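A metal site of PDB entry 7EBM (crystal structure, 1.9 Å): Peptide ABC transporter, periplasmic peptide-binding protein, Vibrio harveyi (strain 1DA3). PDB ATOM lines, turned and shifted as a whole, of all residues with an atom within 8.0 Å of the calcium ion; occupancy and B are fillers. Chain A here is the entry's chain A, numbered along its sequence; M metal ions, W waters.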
ATOM      1  N   LYS A 339      19.806   9.797   8.829  1.00  0.00           N
ATOM      2  CA  LYS A 339      21.075   9.514   8.177  1.00  0.00           C
ATOM      3  C   LYS A 339      21.595  10.742   7.451  1.00  0.00           C
ATOM      4  O   LYS A 339      20.822  11.427   6.780  1.00  0.00           O
ATOM      5  CB  LYS A 339      20.887   8.350   7.196  1.00  0.00           C
ATOM      6  CG  LYS A 339      22.058   8.078   6.277  1.00  0.00           C
ATOM      7  CD  LYS A 339      21.635   7.090   5.195  1.00  0.00           C
ATOM      8  CE  LYS A 339      22.827   6.556   4.458  1.00  0.00           C
ATOM      9  NZ  LYS A 339      23.799   5.956   5.417  1.00  0.00           N
ATOM     10  N   ASP A 340      22.892  11.031   7.591  1.00  0.00           N
ATOM     11  CA  ASP A 340      23.528  12.105   6.815  1.00  0.00           C
ATOM     12  C   ASP A 340      23.750  11.677   5.378  1.00  0.00           C
ATOM     13  O   ASP A 340      24.628  10.853   5.096  1.00  0.00           O
ATOM     14  CB  ASP A 340      24.882  12.524   7.411  1.00  0.00           C
ATOM     15  CG  ASP A 340      25.575  13.619   6.575  1.00  0.00           C
ATOM     16  OD1 ASP A 340      24.879  14.425   5.919  1.00  0.00           O
ATOM     17  OD2 ASP A 340      26.823  13.683   6.583  1.00  0.00           O
ATOM     18  N   VAL A 341      22.968  12.252   4.466  1.00  0.00           N
ATOM     19  CA  VAL A 341      23.025  11.890   3.067  1.00  0.00           C
ATOM     20  C   VAL A 341      23.556  12.990   2.138  1.00  0.00           C
ATOM     21  O   VAL A 341      23.472  12.864   0.925  1.00  0.00           O
ATOM     22  CB  VAL A 341      21.628  11.490   2.560  1.00  0.00           C
ATOM     23  CG1 VAL A 341      21.138  10.226   3.301  1.00  0.00           C
ATOM     24  CG2 VAL A 341      20.658  12.632   2.733  1.00  0.00           C
ATOM     25  N   ASN A 342      24.090  14.081   2.691  1.00  0.00           N
ATOM     26  CA  ASN A 342      24.746  15.055   1.811  1.00  0.00           C
ATOM     27  C   ASN A 342      26.170  15.392   2.274  1.00  0.00           C
ATOM     28  O   ASN A 342      26.727  16.422   1.899  1.00  0.00           O
ATOM     29  CB  ASN A 342      23.894  16.330   1.667  1.00  0.00           C
ATOM     30  CG  ASN A 342      23.694  17.060   2.976  1.00  0.00           C
ATOM     31  OD1 ASN A 342      23.881  16.498   4.035  1.00  0.00           O
ATOM     32  ND2 ASN A 342      23.307  18.330   2.890  1.00  0.00           N
ATOM     33  N   LYS A 343      26.748  14.491   3.063  1.00  0.00           N
ATOM     34  CA  LYS A 343      28.173  14.499   3.406  1.00  0.00           C
ATOM     35  C   LYS A 343      28.653  15.702   4.232  1.00  0.00           C
ATOM     36  O   LYS A 343      29.841  16.009   4.219  1.00  0.00           O
ATOM     37  CB  LYS A 343      29.010  14.428   2.129  1.00  0.00           C
ATOM     38  CG  LYS A 343      28.634  13.316   1.161  1.00  0.00           C
ATOM     39  CD  LYS A 343      29.694  13.172   0.068  1.00  0.00           C
ATOM     40  CE  LYS A 343      29.164  12.417  -1.150  1.00  0.00           C
ATOM     41  NZ  LYS A 343      27.885  12.968  -1.688  1.00  0.00           N
ATOM     42  N   ASP A 344      27.761  16.375   4.955  1.00  0.00           N
ATOM     43  CA  ASP A 344      28.202  17.547   5.717  1.00  0.00           C
ATOM     44  C   ASP A 344      28.406  17.209   7.188  1.00  0.00           C
ATOM     45  O   ASP A 344      28.893  18.031   7.956  1.00  0.00           O
ATOM     46  CB  ASP A 344      27.214  18.706   5.537  1.00  0.00           C
ATOM     47  CG  ASP A 344      25.844  18.418   6.152  1.00  0.00           C
ATOM     48  OD1 ASP A 344      25.606  17.264   6.573  1.00  0.00           O
ATOM     49  OD2 ASP A 344      25.018  19.351   6.210  1.00  0.00           O
ATOM     50  N   GLY A 345      28.056  15.997   7.588  1.00  0.00           N
ATOM     51  CA  GLY A 345      28.307  15.546   8.950  1.00  0.00           C
ATOM     52  C   GLY A 345      27.116  15.671   9.874  1.00  0.00           C
ATOM     53  O   GLY A 345      27.158  15.201  11.009  1.00  0.00           O
ATOM     54  N   PHE A 346      26.048  16.300   9.389  1.00  0.00           N
ATOM     55  CA  PHE A 346      24.815  16.442  10.157  1.00  0.00           C
ATOM     56  C   PHE A 346      23.741  15.514   9.618  1.00  0.00           C
ATOM     57  O   PHE A 346      23.568  15.389   8.411  1.00  0.00           O
ATOM     58  CB  PHE A 346      24.326  17.892  10.119  1.00  0.00           C
ATOM     59  CG  PHE A 346      25.285  18.854  10.750  1.00  0.00           C
ATOM     60  CD1 PHE A 346      25.350  18.973  12.139  1.00  0.00           C
ATOM     61  CD2 PHE A 346      26.125  19.621   9.971  1.00  0.00           C
ATOM     62  CE1 PHE A 346      26.242  19.841  12.732  1.00  0.00           C
ATOM     63  CE2 PHE A 346      27.026  20.507  10.562  1.00  0.00           C
ATOM     64  CZ  PHE A 346      27.084  20.617  11.943  1.00  0.00           C
ATOM     65  N   VAL A 347      23.014  14.859  10.507  1.00  0.00           N
ATOM     66  CA  VAL A 347      21.969  13.972  10.074  1.00  0.00           C
ATOM     67  C   VAL A 347      20.860  14.733   9.351  1.00  0.00           C
ATOM     68  O   VAL A 347      20.623  15.915   9.605  1.00  0.00           O
ATOM     69  CB  VAL A 347      21.355  13.198  11.249  1.00  0.00           C
ATOM     70  CG1 VAL A 347      22.440  12.451  11.986  1.00  0.00           C
ATOM     71  CG2 VAL A 347      20.621  14.163  12.194  1.00  0.00           C
ATOM     72  N   ASP A 348      20.216  14.054   8.427  1.00  0.00           N
ATOM     73  CA  ASP A 348      19.078  14.605   7.712  1.00  0.00           C
ATOM     74  C   ASP A 348      17.845  13.799   8.124  1.00  0.00           C
ATOM     75  O   ASP A 348      18.000  12.785   8.798  1.00  0.00           O
ATOM     76  CB  ASP A 348      19.370  14.552   6.207  1.00  0.00           C
ATOM     77  CG  ASP A 348      20.698  15.260   5.849  1.00  0.00           C
ATOM     78  OD1 ASP A 348      20.835  16.460   6.158  1.00  0.00           O
ATOM     79  OD2 ASP A 348      21.621  14.619   5.273  1.00  0.00           O
ATOM     80  N   THR A 349      16.642  14.239   7.767  1.00  0.00           N
ATOM     81  CA  THR A 349      15.412  13.539   8.137  1.00  0.00           C
ATOM     82  C   THR A 349      15.305  12.189   7.398  1.00  0.00           C
ATOM     83  O   THR A 349      16.041  11.945   6.456  1.00  0.00           O
ATOM     84  CB  THR A 349      14.164  14.379   7.825  1.00  0.00           C
ATOM     85  OG1 THR A 349      14.029  14.483   6.405  1.00  0.00           O
ATOM     86  CG2 THR A 349      14.250  15.785   8.466  1.00  0.00           C
ATOM     87  N   GLY A 352      15.099  12.478   3.774  1.00  0.00           N
ATOM     88  CA  GLY A 352      16.295  12.951   3.108  1.00  0.00           C
ATOM     89  C   GLY A 352      16.558  14.438   3.208  1.00  0.00           C
ATOM     90  O   GLY A 352      17.519  14.938   2.624  1.00  0.00           O
ATOM     91  N   LYS A 353      15.743  15.156   3.977  1.00  0.00           N
ATOM     92  CA  LYS A 353      15.830  16.619   4.058  1.00  0.00           C
ATOM     93  C   LYS A 353      16.812  17.138   5.106  1.00  0.00           C
ATOM     94  O   LYS A 353      16.823  16.673   6.247  1.00  0.00           O
ATOM     95  CB  LYS A 353      14.459  17.199   4.349  1.00  0.00           C
ATOM     96  CG  LYS A 353      13.461  16.943   3.261  1.00  0.00           C
ATOM     97  CD  LYS A 353      12.073  17.249   3.762  1.00  0.00           C
ATOM     98  CE  LYS A 353      11.011  16.798   2.768  1.00  0.00           C
ATOM     99  NZ  LYS A 353       9.754  16.452   3.485  1.00  0.00           N
ATOM    100  N   SER A 354      17.612  18.134   4.718  1.00  0.00           N
ATOM    101  CA  SER A 354      18.511  18.796   5.648  1.00  0.00           C
ATOM    102  C   SER A 354      17.706  19.672   6.586  1.00  0.00           C
ATOM    103  O   SER A 354      16.623  20.120   6.237  1.00  0.00           O
ATOM    104  CB  SER A 354      19.549  19.646   4.904  1.00  0.00           C
ATOM    105  OG  SER A 354      20.661  18.848   4.509  1.00  0.00           O
ATOM    106  N   PHE A 355      18.220  19.904   7.782  1.00  0.00           N
ATOM    107  CA  PHE A 355      17.495  20.792   8.685  1.00  0.00           C
ATOM    108  C   PHE A 355      18.413  21.326   9.775  1.00  0.00           C
ATOM    109  O   PHE A 355      19.413  20.705  10.109  1.00  0.00           O
ATOM    110  CB  PHE A 355      16.279  20.077   9.307  1.00  0.00           C
ATOM    111  CG  PHE A 355      16.653  18.971  10.267  1.00  0.00           C
ATOM    112  CD1 PHE A 355      16.639  19.185  11.639  1.00  0.00           C
ATOM    113  CD2 PHE A 355      17.018  17.713   9.798  1.00  0.00           C
ATOM    114  CE1 PHE A 355      16.986  18.163  12.522  1.00  0.00           C
ATOM    115  CE2 PHE A 355      17.362  16.690  10.661  1.00  0.00           C
ATOM    116  CZ  PHE A 355      17.352  16.913  12.032  1.00  0.00           C
ATOM    117  N   GLY A 383      25.768  14.909  15.590  1.00  0.00           N
ATOM    118  CA  GLY A 383      25.335  15.170  14.222  1.00  0.00           C
ATOM    119  C   GLY A 383      24.021  15.901  14.055  1.00  0.00           C
ATOM    120  O   GLY A 383      23.470  15.934  12.955  1.00  0.00           O
ATOM    121  N   LYS A 385      22.192  19.396  13.799  1.00  0.00           N
ATOM    122  CA  LYS A 385      22.528  20.775  13.532  1.00  0.00           C
ATOM    123  C   LYS A 385      21.592  21.740  14.239  1.00  0.00           C
ATOM    124  O   LYS A 385      20.378  21.717  14.031  1.00  0.00           O
ATOM    125  CB  LYS A 385      22.508  21.061  12.029  1.00  0.00           C
ATOM    126  CG  LYS A 385      23.047  22.449  11.654  1.00  0.00           C
ATOM    127  CD  LYS A 385      23.333  22.557  10.148  1.00  0.00           C
ATOM    128  CE  LYS A 385      24.140  23.813   9.808  1.00  0.00           C
ATOM    129  NZ  LYS A 385      23.404  25.099  10.028  1.00  0.00           N
HETATM  130 CA    CA M   1      23.345  16.245   6.186  1.00  0.00          CA
HETATM  131  O   HOH W   1      22.707  18.456   6.675  1.00  0.00           O
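The side-chain amide nitrogen of Asn 342 sits at hydrogen-bond distance from the side-chain hydroxyl of Ser 354 (3.1 Å).
The backbone NH of Gly 345 lies within hydrogen-bond range of the side-chain carboxylate of Asp 340 (2.8 Å).
OD1 of Asp 340 lies close to N of Lys 343, 3.4 Å away.
The side-chain carboxylate (OD1) of Asp 348 lies close to the side-chain hydroxyl (OG) of Ser 354, 2.9 Å away.
OD2 of Asp 348 lies close to N of Val 341 (2.8 Å).
The backbone carbonyl oxygen (O) of Lys 339 lies within hydrogen-bond range of the backbone NH (N) of Asp 348, at 3.2 Å.
The nearest printed residue that does not touch the calcium ion is Ser 354 (4.1 Å).
OD1 of Asn 342 is bound to the calcium ion, at 2.2 Å.
Water W1 is bound to the calcium ion, 2.4 Å away.
The calcium ion is bound by O of Phe 346, at 2.4 Å.
OD1 of Asp 340 binds the calcium ion, 2.4 Å away.
The calcium ion is bound by OD1 of Asp 344 (2.5 Å).
OD1 of Asp 348 is bound to the calcium ion (2.5 Å).
The calcium ion is bound by OD2 of Asp 348 (2.5 Å).
The calcium ion has seven donor atoms within binding distance.
Water W1 lies within hydrogen-bond range of the side-chain carboxylate (OD2) of Asp 344 (2.5 Å) and the side-chain hydroxyl (OG) of Ser 354 (3.0 Å).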
